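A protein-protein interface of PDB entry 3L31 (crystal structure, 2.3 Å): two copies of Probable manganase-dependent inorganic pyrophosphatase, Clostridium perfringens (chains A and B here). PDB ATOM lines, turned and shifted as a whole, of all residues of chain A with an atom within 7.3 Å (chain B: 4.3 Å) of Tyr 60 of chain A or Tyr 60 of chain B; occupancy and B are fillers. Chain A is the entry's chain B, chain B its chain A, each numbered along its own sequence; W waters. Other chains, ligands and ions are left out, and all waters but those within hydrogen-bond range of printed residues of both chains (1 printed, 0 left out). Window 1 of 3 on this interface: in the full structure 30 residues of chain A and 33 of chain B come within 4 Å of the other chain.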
ATOM      1  N   LEU A  23     -18.925  18.057  14.516  1.00  0.00           N
ATOM      2  CA  LEU A  23     -18.142  17.273  13.548  1.00  0.00           C
ATOM      3  C   LEU A  23     -16.672  17.341  13.867  1.00  0.00           C
ATOM      4  O   LEU A  23     -15.922  16.359  13.777  1.00  0.00           O
ATOM      5  CB  LEU A  23     -18.421  17.691  12.085  1.00  0.00           C
ATOM      6  CG  LEU A  23     -19.864  17.530  11.586  1.00  0.00           C
ATOM      7  CD1 LEU A  23     -20.025  17.858  10.109  1.00  0.00           C
ATOM      8  CD2 LEU A  23     -20.427  16.130  11.881  1.00  0.00           C
ATOM      9  N   TRP A  27     -14.598  14.107  14.654  1.00  0.00           N
ATOM     10  CA  TRP A  27     -13.435  13.767  13.860  1.00  0.00           C
ATOM     11  C   TRP A  27     -12.170  13.602  14.721  1.00  0.00           C
ATOM     12  O   TRP A  27     -11.397  12.657  14.528  1.00  0.00           O
ATOM     13  CB  TRP A  27     -13.233  14.804  12.764  1.00  0.00           C
ATOM     14  CG  TRP A  27     -11.994  14.635  12.063  1.00  0.00           C
ATOM     15  CD1 TRP A  27     -10.923  15.436  12.132  1.00  0.00           C
ATOM     16  CD2 TRP A  27     -11.672  13.599  11.173  1.00  0.00           C
ATOM     17  NE1 TRP A  27      -9.939  14.972  11.341  1.00  0.00           N
ATOM     18  CE2 TRP A  27     -10.373  13.833  10.731  1.00  0.00           C
ATOM     19  CE3 TRP A  27     -12.346  12.467  10.724  1.00  0.00           C
ATOM     20  CZ2 TRP A  27      -9.719  12.991   9.854  1.00  0.00           C
ATOM     21  CZ3 TRP A  27     -11.698  11.631   9.841  1.00  0.00           C
ATOM     22  CH2 TRP A  27     -10.395  11.892   9.423  1.00  0.00           C
ATOM     23  N   SER A  54     -17.493   9.227   5.704  1.00  0.00           N
ATOM     24  CA  SER A  54     -18.145   9.620   4.455  1.00  0.00           C
ATOM     25  C   SER A  54     -19.228  10.644   4.694  1.00  0.00           C
ATOM     26  O   SER A  54     -19.458  11.490   3.842  1.00  0.00           O
ATOM     27  CB  SER A  54     -18.670   8.449   3.611  1.00  0.00           C
ATOM     28  OG  SER A  54     -18.682   7.197   4.287  1.00  0.00           O
ATOM     29  N   ASN A  55     -19.870  10.576   5.864  1.00  0.00           N
ATOM     30  CA  ASN A  55     -21.012  11.412   6.159  1.00  0.00           C
ATOM     31  C   ASN A  55     -20.502  12.801   6.470  1.00  0.00           C
ATOM     32  O   ASN A  55     -21.175  13.794   6.228  1.00  0.00           O
ATOM     33  CB  ASN A  55     -21.791  10.931   7.388  1.00  0.00           C
ATOM     34  CG  ASN A  55     -22.431   9.556   7.214  1.00  0.00           C
ATOM     35  OD1 ASN A  55     -22.229   8.693   8.053  1.00  0.00           O
ATOM     36  ND2 ASN A  55     -23.222   9.358   6.142  1.00  0.00           N
ATOM     37  N   ILE A  56     -19.322  12.853   7.077  1.00  0.00           N
ATOM     38  CA  ILE A  56     -18.656  14.123   7.367  1.00  0.00           C
ATOM     39  C   ILE A  56     -18.180  14.772   6.073  1.00  0.00           C
ATOM     40  O   ILE A  56     -18.476  15.930   5.787  1.00  0.00           O
ATOM     41  CB  ILE A  56     -17.425  13.903   8.244  1.00  0.00           C
ATOM     42  CG1 ILE A  56     -17.871  13.397   9.600  1.00  0.00           C
ATOM     43  CG2 ILE A  56     -16.594  15.160   8.364  1.00  0.00           C
ATOM     44  CD1 ILE A  56     -16.736  13.079  10.542  1.00  0.00           C
ATOM     45  N   THR A  57     -17.421  14.019   5.309  1.00  0.00           N
ATOM     46  CA  THR A  57     -16.928  14.513   4.029  1.00  0.00           C
ATOM     47  C   THR A  57     -18.075  15.024   3.132  1.00  0.00           C
ATOM     48  O   THR A  57     -18.058  16.182   2.674  1.00  0.00           O
ATOM     49  CB  THR A  57     -16.145  13.438   3.279  1.00  0.00           C
ATOM     50  OG1 THR A  57     -15.272  12.739   4.176  1.00  0.00           O
ATOM     51  CG2 THR A  57     -15.358  14.046   2.149  1.00  0.00           C
ATOM     52  N   ALA A  58     -19.057  14.163   2.871  1.00  0.00           N
ATOM     53  CA  ALA A  58     -20.233  14.583   2.065  1.00  0.00           C
ATOM     54  C   ALA A  58     -20.779  15.912   2.564  1.00  0.00           C
ATOM     55  O   ALA A  58     -21.188  16.761   1.762  1.00  0.00           O
ATOM     56  CB  ALA A  58     -21.351  13.532   2.024  1.00  0.00           C
ATOM     57  N   THR A  59     -20.736  16.129   3.868  1.00  0.00           N
ATOM     58  CA  THR A  59     -21.284  17.374   4.430  1.00  0.00           C
ATOM     59  C   THR A  59     -20.463  18.588   4.022  1.00  0.00           C
ATOM     60  O   THR A  59     -21.005  19.672   3.824  1.00  0.00           O
ATOM     61  CB  THR A  59     -21.418  17.368   5.983  1.00  0.00           C
ATOM     62  OG1 THR A  59     -22.319  16.330   6.400  1.00  0.00           O
ATOM     63  CG2 THR A  59     -21.943  18.712   6.474  1.00  0.00           C
ATOM     64  N   TYR A  60     -19.154  18.396   3.874  1.00  0.00           N
ATOM     65  CA  TYR A  60     -18.257  19.513   3.529  1.00  0.00           C
ATOM     66  C   TYR A  60     -18.244  19.753   2.042  1.00  0.00           C
ATOM     67  O   TYR A  60     -18.271  20.885   1.612  1.00  0.00           O
ATOM     68  CB  TYR A  60     -16.816  19.297   4.025  1.00  0.00           C
ATOM     69  CG  TYR A  60     -15.941  20.539   3.912  1.00  0.00           C
ATOM     70  CD1 TYR A  60     -15.418  21.155   5.045  1.00  0.00           C
ATOM     71  CD2 TYR A  60     -15.657  21.109   2.674  1.00  0.00           C
ATOM     72  CE1 TYR A  60     -14.633  22.286   4.949  1.00  0.00           C
ATOM     73  CE2 TYR A  60     -14.866  22.255   2.564  1.00  0.00           C
ATOM     74  CZ  TYR A  60     -14.354  22.839   3.703  1.00  0.00           C
ATOM     75  OH  TYR A  60     -13.559  23.971   3.615  1.00  0.00           O
ATOM     76  N   MET A  61     -18.185  18.680   1.268  1.00  0.00           N
ATOM     77  CA  MET A  61     -18.101  18.772  -0.213  1.00  0.00           C
ATOM     78  C   MET A  61     -19.417  19.272  -0.842  1.00  0.00           C
ATOM     79  O   MET A  61     -19.493  20.376  -1.392  1.00  0.00           O
ATOM     80  CB  MET A  61     -17.737  17.407  -0.834  1.00  0.00           C
ATOM     81  CG  MET A  61     -16.449  16.745  -0.292  1.00  0.00           C
ATOM     82  SD  MET A  61     -14.921  17.732  -0.427  1.00  0.00           S
ATOM     83  CE  MET A  61     -14.657  17.763  -2.183  1.00  0.00           C
ATOM     84  N   ASP A  62     -20.433  18.415  -0.747  1.00  0.00           N
ATOM     85  CA  ASP A  62     -21.818  18.674  -1.216  1.00  0.00           C
ATOM     86  C   ASP A  62     -22.643  19.596  -0.276  1.00  0.00           C
ATOM     87  O   ASP A  62     -23.616  19.137   0.366  1.00  0.00           O
ATOM     88  CB  ASP A  62     -22.586  17.341  -1.337  1.00  0.00           C
ATOM     89  CG  ASP A  62     -21.815  16.287  -2.114  1.00  0.00           C
ATOM     90  OD1 ASP A  62     -21.069  16.707  -3.032  1.00  0.00           O
ATOM     91  OD2 ASP A  62     -21.936  15.065  -1.815  1.00  0.00           O
ATOM     92  N   ILE A  63     -22.305  20.878  -0.174  1.00  0.00           N
ATOM     93  CA  ILE A  63     -23.224  21.780   0.536  1.00  0.00           C
ATOM     94  C   ILE A  63     -23.384  23.129  -0.135  1.00  0.00           C
ATOM     95  O   ILE A  63     -22.437  23.932  -0.289  1.00  0.00           O
ATOM     96  CB  ILE A  63     -22.875  21.979   2.036  1.00  0.00           C
ATOM     97  N   TRP A  64     -24.627  23.360  -0.520  1.00  0.00           N
ATOM     98  CA  TRP A  64     -25.052  24.660  -0.993  1.00  0.00           C
ATOM     99  C   TRP A  64     -25.884  25.322   0.118  1.00  0.00           C
ATOM    100  O   TRP A  64     -25.897  26.550   0.310  1.00  0.00           O
ATOM    101  CB  TRP A  64     -25.897  24.477  -2.263  1.00  0.00           C
ATOM    102  N   PHE A 172     -11.614  34.396   6.115  1.00  0.00           N
ATOM    103  CA  PHE A 172     -11.509  33.200   5.260  1.00  0.00           C
ATOM    104  C   PHE A 172     -11.580  31.938   6.081  1.00  0.00           C
ATOM    105  O   PHE A 172     -12.267  30.954   5.723  1.00  0.00           O
ATOM    106  CB  PHE A 172     -10.196  33.243   4.421  1.00  0.00           C
ATOM    107  CG  PHE A 172      -9.846  31.949   3.732  1.00  0.00           C
ATOM    108  CD1 PHE A 172     -10.594  31.495   2.636  1.00  0.00           C
ATOM    109  CD2 PHE A 172      -8.749  31.230   4.120  1.00  0.00           C
ATOM    110  CE1 PHE A 172     -10.288  30.330   2.005  1.00  0.00           C
ATOM    111  CE2 PHE A 172      -8.380  30.041   3.487  1.00  0.00           C
ATOM    112  CZ  PHE A 172      -9.137  29.582   2.428  1.00  0.00           C
ATOM    113  N   SER A 175     -14.842  31.200   7.862  1.00  0.00           N
ATOM    114  CA  SER A 175     -15.824  30.665   6.875  1.00  0.00           C
ATOM    115  C   SER A 175     -15.571  29.131   6.628  1.00  0.00           C
ATOM    116  O   SER A 175     -16.525  28.340   6.506  1.00  0.00           O
ATOM    117  CB  SER A 175     -15.752  31.451   5.563  1.00  0.00           C
ATOM    118  OG  SER A 175     -16.043  32.850   5.727  1.00  0.00           O
ATOM    119  N   ARG A 176     -14.287  28.723   6.629  1.00  0.00           N
ATOM    120  CA  ARG A 176     -13.917  27.306   6.461  1.00  0.00           C
ATOM    121  C   ARG A 176     -14.253  26.490   7.689  1.00  0.00           C
ATOM    122  O   ARG A 176     -14.505  25.314   7.608  1.00  0.00           O
ATOM    123  CB  ARG A 176     -12.427  27.112   6.215  1.00  0.00           C
ATOM    124  CG  ARG A 176     -11.925  27.481   4.842  1.00  0.00           C
ATOM    125  CD  ARG A 176     -10.478  27.037   4.706  1.00  0.00           C
ATOM    126  NE  ARG A 176     -10.309  25.627   5.028  1.00  0.00           N
ATOM    127  CZ  ARG A 176      -9.144  24.982   4.950  1.00  0.00           C
ATOM    128  NH1 ARG A 176      -8.030  25.609   4.545  1.00  0.00           N
ATOM    129  NH2 ARG A 176      -9.092  23.685   5.257  1.00  0.00           N
ATOM    130  N   LEU A 177     -14.238  27.117   8.840  1.00  0.00           N
ATOM    131  CA  LEU A 177     -14.314  26.347  10.064  1.00  0.00           C
ATOM    132  C   LEU A 177     -15.744  26.156  10.463  1.00  0.00           C
ATOM    133  O   LEU A 177     -16.129  25.123  11.024  1.00  0.00           O
ATOM    134  CB  LEU A 177     -13.548  27.012  11.247  1.00  0.00           C
ATOM    135  CG  LEU A 177     -12.055  26.745  11.319  1.00  0.00           C
ATOM    136  CD1 LEU A 177     -11.407  27.702  12.244  1.00  0.00           C
ATOM    137  CD2 LEU A 177     -11.752  25.250  11.751  1.00  0.00           C
ATOM    138  N   VAL A 179     -18.472  25.349   9.419  1.00  0.00           N
ATOM    139  CA  VAL A 179     -19.379  24.261   9.053  1.00  0.00           C
ATOM    140  C   VAL A 179     -19.042  23.006   9.870  1.00  0.00           C
ATOM    141  O   VAL A 179     -19.844  22.085   9.991  1.00  0.00           O
ATOM    142  CB  VAL A 179     -19.394  23.972   7.534  1.00  0.00           C
ATOM    143  CG1 VAL A 179     -19.938  22.570   7.252  1.00  0.00           C
ATOM    144  CG2 VAL A 179     -20.236  25.052   6.790  1.00  0.00           C
ATOM    145  N   GLN A 180     -17.869  23.012  10.473  1.00  0.00           N
ATOM    146  CA  GLN A 180     -17.450  21.902  11.319  1.00  0.00           C
ATOM    147  C   GLN A 180     -18.191  21.860  12.657  1.00  0.00           C
ATOM    148  O   GLN A 180     -18.027  20.923  13.441  1.00  0.00           O
ATOM    149  CB  GLN A 180     -15.951  21.963  11.556  1.00  0.00           C
ATOM    150  CG  GLN A 180     -15.138  21.842  10.277  1.00  0.00           C
ATOM    151  CD  GLN A 180     -13.639  21.885  10.542  1.00  0.00           C
ATOM    152  OE1 GLN A 180     -13.204  21.610  11.649  1.00  0.00           O
ATOM    153  NE2 GLN A 180     -12.854  22.295   9.535  1.00  0.00           N
ATOM    154  N   LEU A 182     -21.522  21.617  13.083  1.00  0.00           N
ATOM    155  CA  LEU A 182     -22.772  20.885  13.100  1.00  0.00           C
ATOM    156  C   LEU A 182     -22.698  19.685  14.055  1.00  0.00           C
ATOM    157  O   LEU A 182     -21.637  19.057  14.226  1.00  0.00           O
ATOM    158  CB  LEU A 182     -23.184  20.388  11.699  1.00  0.00           C
ATOM    159  CG  LEU A 182     -23.067  21.395  10.558  1.00  0.00           C
ATOM    160  CD1 LEU A 182     -23.360  20.732   9.220  1.00  0.00           C
ATOM    161  CD2 LEU A 182     -23.957  22.558  10.780  1.00  0.00           C
ATOM    162  N   LEU B  23      -9.715  17.331  -5.403  1.00  0.00           N
ATOM    163  CA  LEU B  23     -10.434  16.626  -4.369  1.00  0.00           C
ATOM    164  C   LEU B  23     -11.885  16.564  -4.794  1.00  0.00           C
ATOM    165  O   LEU B  23     -12.567  15.563  -4.656  1.00  0.00           O
ATOM    166  CB  LEU B  23     -10.300  17.317  -3.022  1.00  0.00           C
ATOM    167  CG  LEU B  23      -8.864  17.339  -2.506  1.00  0.00           C
ATOM    168  CD1 LEU B  23      -8.844  17.870  -1.102  1.00  0.00           C
ATOM    169  CD2 LEU B  23      -8.247  15.937  -2.614  1.00  0.00           C
ATOM    170  N   ILE B  56      -9.181  13.022   2.284  1.00  0.00           N
ATOM    171  CA  ILE B  56      -9.980  14.200   1.929  1.00  0.00           C
ATOM    172  C   ILE B  56     -10.479  14.938   3.205  1.00  0.00           C
ATOM    173  O   ILE B  56     -10.287  16.159   3.395  1.00  0.00           O
ATOM    174  CB  ILE B  56     -11.193  13.799   1.018  1.00  0.00           C
ATOM    175  CG1 ILE B  56     -10.694  13.105  -0.263  1.00  0.00           C
ATOM    176  CG2 ILE B  56     -12.022  15.006   0.673  1.00  0.00           C
ATOM    177  CD1 ILE B  56     -11.805  12.536  -1.164  1.00  0.00           C
ATOM    178  N   THR B  57     -11.110  14.185   4.088  1.00  0.00           N
ATOM    179  CA  THR B  57     -11.642  14.765   5.289  1.00  0.00           C
ATOM    180  C   THR B  57     -10.547  15.426   6.158  1.00  0.00           C
ATOM    181  O   THR B  57     -10.702  16.579   6.578  1.00  0.00           O
ATOM    182  CB  THR B  57     -12.343  13.693   6.137  1.00  0.00           C
ATOM    183  OG1 THR B  57     -13.172  12.882   5.298  1.00  0.00           O
ATOM    184  CG2 THR B  57     -13.152  14.308   7.219  1.00  0.00           C
ATOM    185  N   ALA B  58      -9.469  14.716   6.462  1.00  0.00           N
ATOM    186  CA  ALA B  58      -8.395  15.370   7.232  1.00  0.00           C
ATOM    187  C   ALA B  58      -8.002  16.691   6.587  1.00  0.00           C
ATOM    188  O   ALA B  58      -7.708  17.651   7.280  1.00  0.00           O
ATOM    189  CB  ALA B  58      -7.161  14.482   7.427  1.00  0.00           C
ATOM    190  N   THR B  59      -8.017  16.764   5.267  1.00  0.00           N
ATOM    191  CA  THR B  59      -7.550  17.997   4.608  1.00  0.00           C
ATOM    192  C   THR B  59      -8.428  19.207   4.932  1.00  0.00           C
ATOM    193  O   THR B  59      -7.947  20.340   5.053  1.00  0.00           O
ATOM    194  CB  THR B  59      -7.431  17.846   3.090  1.00  0.00           C
ATOM    195  OG1 THR B  59      -6.481  16.812   2.780  1.00  0.00           O
ATOM    196  CG2 THR B  59      -6.977  19.159   2.481  1.00  0.00           C
ATOM    197  N   TYR B  60      -9.720  18.971   5.089  1.00  0.00           N
ATOM    198  CA  TYR B  60     -10.633  20.042   5.484  1.00  0.00           C
ATOM    199  C   TYR B  60     -10.544  20.326   6.965  1.00  0.00           C
ATOM    200  O   TYR B  60     -10.382  21.461   7.388  1.00  0.00           O
ATOM    201  CB  TYR B  60     -12.059  19.655   5.153  1.00  0.00           C
ATOM    202  CG  TYR B  60     -12.216  19.306   3.713  1.00  0.00           C
ATOM    203  CD1 TYR B  60     -11.628  20.082   2.733  1.00  0.00           C
ATOM    204  CD2 TYR B  60     -12.947  18.208   3.332  1.00  0.00           C
ATOM    205  CE1 TYR B  60     -11.759  19.768   1.412  1.00  0.00           C
ATOM    206  CE2 TYR B  60     -13.088  17.886   2.023  1.00  0.00           C
ATOM    207  CZ  TYR B  60     -12.494  18.665   1.060  1.00  0.00           C
ATOM    208  OH  TYR B  60     -12.645  18.353  -0.268  1.00  0.00           O
ATOM    209  N   MET B  61     -10.645  19.272   7.750  1.00  0.00           N
ATOM    210  CA  MET B  61     -10.744  19.412   9.222  1.00  0.00           C
ATOM    211  C   MET B  61      -9.461  19.885   9.915  1.00  0.00           C
ATOM    212  O   MET B  61      -9.472  20.225  11.112  1.00  0.00           O
ATOM    213  CB  MET B  61     -11.156  18.068   9.869  1.00  0.00           C
ATOM    214  CG  MET B  61     -12.378  17.406   9.245  1.00  0.00           C
ATOM    215  SD  MET B  61     -13.843  18.424   9.418  1.00  0.00           S
ATOM    216  CE  MET B  61     -14.029  18.333  11.204  1.00  0.00           C
ATOM    217  N   ASP B  62      -8.351  19.871   9.190  1.00  0.00           N
ATOM    218  CA  ASP B  62      -7.026  20.106   9.802  1.00  0.00           C
ATOM    219  C   ASP B  62      -6.167  21.033   8.936  1.00  0.00           C
ATOM    220  O   ASP B  62      -5.267  20.575   8.201  1.00  0.00           O
ATOM    221  CB  ASP B  62      -6.271  18.775  10.007  1.00  0.00           C
ATOM    222  CG  ASP B  62      -6.968  17.840  10.973  1.00  0.00           C
ATOM    223  OD1 ASP B  62      -7.564  18.343  11.950  1.00  0.00           O
ATOM    224  OD2 ASP B  62      -6.903  16.600  10.782  1.00  0.00           O
ATOM    225  N   ARG B 176     -15.413  28.424   1.380  1.00  0.00           N
ATOM    226  CA  ARG B 176     -15.628  27.007   1.715  1.00  0.00           C
ATOM    227  C   ARG B 176     -15.221  26.094   0.581  1.00  0.00           C
ATOM    228  O   ARG B 176     -14.858  24.954   0.794  1.00  0.00           O
ATOM    229  CB  ARG B 176     -17.098  26.700   2.020  1.00  0.00           C
ATOM    230  CG  ARG B 176     -17.648  27.297   3.351  1.00  0.00           C
ATOM    231  CD  ARG B 176     -19.129  26.963   3.530  1.00  0.00           C
ATOM    232  NE  ARG B 176     -19.372  25.525   3.450  1.00  0.00           N
ATOM    233  CZ  ARG B 176     -20.591  24.980   3.406  1.00  0.00           C
ATOM    234  NH1 ARG B 176     -21.679  25.752   3.413  1.00  0.00           N
ATOM    235  NH2 ARG B 176     -20.730  23.654   3.354  1.00  0.00           N
ATOM    236  N   VAL B 179     -10.823  25.050  -1.140  1.00  0.00           N
ATOM    237  CA  VAL B 179      -9.939  23.966  -0.706  1.00  0.00           C
ATOM    238  C   VAL B 179     -10.241  22.625  -1.413  1.00  0.00           C
ATOM    239  O   VAL B 179      -9.418  21.735  -1.444  1.00  0.00           O
ATOM    240  CB  VAL B 179      -9.874  23.868   0.792  1.00  0.00           C
ATOM    241  CG1 VAL B 179      -9.134  22.562   1.256  1.00  0.00           C
ATOM    242  CG2 VAL B 179      -9.115  25.114   1.312  1.00  0.00           C
ATOM    243  N   GLN B 180     -11.380  22.557  -2.093  1.00  0.00           N
ATOM    244  CA  GLN B 180     -11.725  21.419  -2.934  1.00  0.00           C
ATOM    245  C   GLN B 180     -10.959  21.320  -4.231  1.00  0.00           C
ATOM    246  O   GLN B 180     -11.062  20.303  -4.954  1.00  0.00           O
ATOM    247  CB  GLN B 180     -13.238  21.418  -3.233  1.00  0.00           C
ATOM    248  CG  GLN B 180     -13.961  21.341  -1.917  1.00  0.00           C
ATOM    249  CD  GLN B 180     -15.428  21.225  -2.070  1.00  0.00           C
ATOM    250  OE1 GLN B 180     -15.926  20.805  -3.121  1.00  0.00           O
ATOM    251  NE2 GLN B 180     -16.161  21.629  -1.014  1.00  0.00           N
HETATM  252  O   HOH W   1     -20.032  25.074   0.050  1.00  0.00           O
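Among the printed residues, merely in contact across the chains: Leu 23 of chain A with Met 61 of chain B (3.8 Å), Trp 27 of chain A with Ala 58 of chain B (3.8 Å), Trp 27 of chain A with Met 61 of chain B (3.5 Å), Ile 56 of chain A with Thr 57 of chain B (3.7 Å), Thr 57 of chain A with Ile 56 of chain B (3.8 Å), Tyr 60 of chain A with Tyr 60 of chain B (3.7 Å), Met 61 of chain A with Leu 23 of chain B (3.9 Å), Met 61 of chain A with Gln 180 of chain B (3.4 Å), Ile 63 of chain A with Arg 176 of chain B (3.0 Å), Ser 175 of chain A with Arg 176 of chain B (3.5 Å), Arg 176 of chain A with Thr 59 of chain B (3.5 Å), Arg 176 of chain A with Val 179 of chain B (3.4 Å), Val 179 of chain A with Arg 176 of chain B (3.4 Å) and Gln 180 of chain A with Met 61 of chain B (3.4 Å).
Of the printed residues of chain B, Thr 57 of chain A touches Ile 56 and Thr 57.
Printed residues of chain B within 4 Å of Met 61 of chain A: Leu 23 (3.9 Å), Tyr 60 (2.4 Å) and Gln 180 (3.4 Å).
Of the printed residues of chain A, Ala 58 of chain B touches Trp 27 (3.8 Å).
Of the printed residues of chain A, Thr 59 of chain B touches Arg 176.
Of the printed residues of chain A, Asp 62 of chain B touches Trp 27 (3.5 Å).
The nearest printed residue of chain B that does not touch Tyr 60 of chain A is Val 179 of chain B (4.6 Å).
The nearest printed residue of chain A that does not touch Tyr 60 of chain B is Thr 57 of chain A (4.5 Å).
The nearest printed residue of chain B that does not touch Thr 57 of chain A is Tyr 60 of chain B (4.5 Å).
Thr 57 of chain A touches its own counterpart, Thr 57 of chain B.
Tyr 60 of chain A touches its own counterpart, Tyr 60 of chain B.
Tyr 60 of chain A touches Gln 180 of chain B, and with the chains exchanged Gln 180 of chain A touches Tyr 60 of chain B.
Met 61 of chain A touches Gln 180 of chain B, and with the chains exchanged Gln 180 of chain A touches Met 61 of chain B.
Positions printed for both chains: 23, 56, 57, 58, 59, 60, 61, 62, 176, 179 and 180.
Of the 11 printed residues of chain B, 11 touch a printed residue of chain A.
Printed residues of chain B that touch a printed residue of chain A: Leu 23, Ile 56, Thr 57, Ala 58, Thr 59, Tyr 60, Met 61, Asp 62, Arg 176, Val 179 and Gln 180.
Hydrophobic or aromatic side chains of chain B within 4 Å of the printed part of chain A: Ile 56, Ala 58, Tyr 60, Met 61 and Val 179.
Among the printed residues, 21 pairs touch across the chains.
Among the printed residues, no Asp or Glu carboxylate lies within 4 Å of a Lys or Arg side-chain nitrogen of the other chain.
Water W1 bridges O of Ile 63 of chain A (2.7 Å) and NE of Arg 176 of chain B (3.5 Å).
NE1 of Trp 27 of chain A lies within hydrogen-bond range of OD2 of Asp 62 of chain B, at 3.5 Å.
The side-chain hydroxyl of Thr 57 of chain A sits close to the side-chain hydroxyl of Thr 57 of chain B, 2.4 Å away.
The backbone carbonyl oxygen of Tyr 60 of chain A lies within hydrogen-bond range of the side-chain amide nitrogen of Gln 180 of chain B, at 3.4 Å.
SD of Met 61 of chain A sits close to OH of Tyr 60 of chain B, at 2.4 Å.
The backbone carbonyl oxygen (O) of Arg 176 of chain B sits close to the side-chain hydroxyl (OH) of Tyr 60 of chain A (3.3 Å).
NE2 of Gln 180 of chain A is in hydrogen-bond range of O of Tyr 60 of chain B, 3.4 Å away.
The backbone carbonyl oxygen of Tyr 60 of chain B is in hydrogen-bond range of the guanidinium group of Arg 176 of chain A, 3.3 Å away.
O of Gln 180 of chain A lies within hydrogen-bond range of N of Leu 23 of chain A.
The backbone NH (N) of Leu 23 of chain A is in hydrogen-bond range of the backbone carbonyl oxygen (O) of Leu 182 of chain A (2.9 Å).
The backbone NH of Leu 23 of chain B sits at hydrogen-bond distance from the backbone carbonyl oxygen of Gln 180 of chain B.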
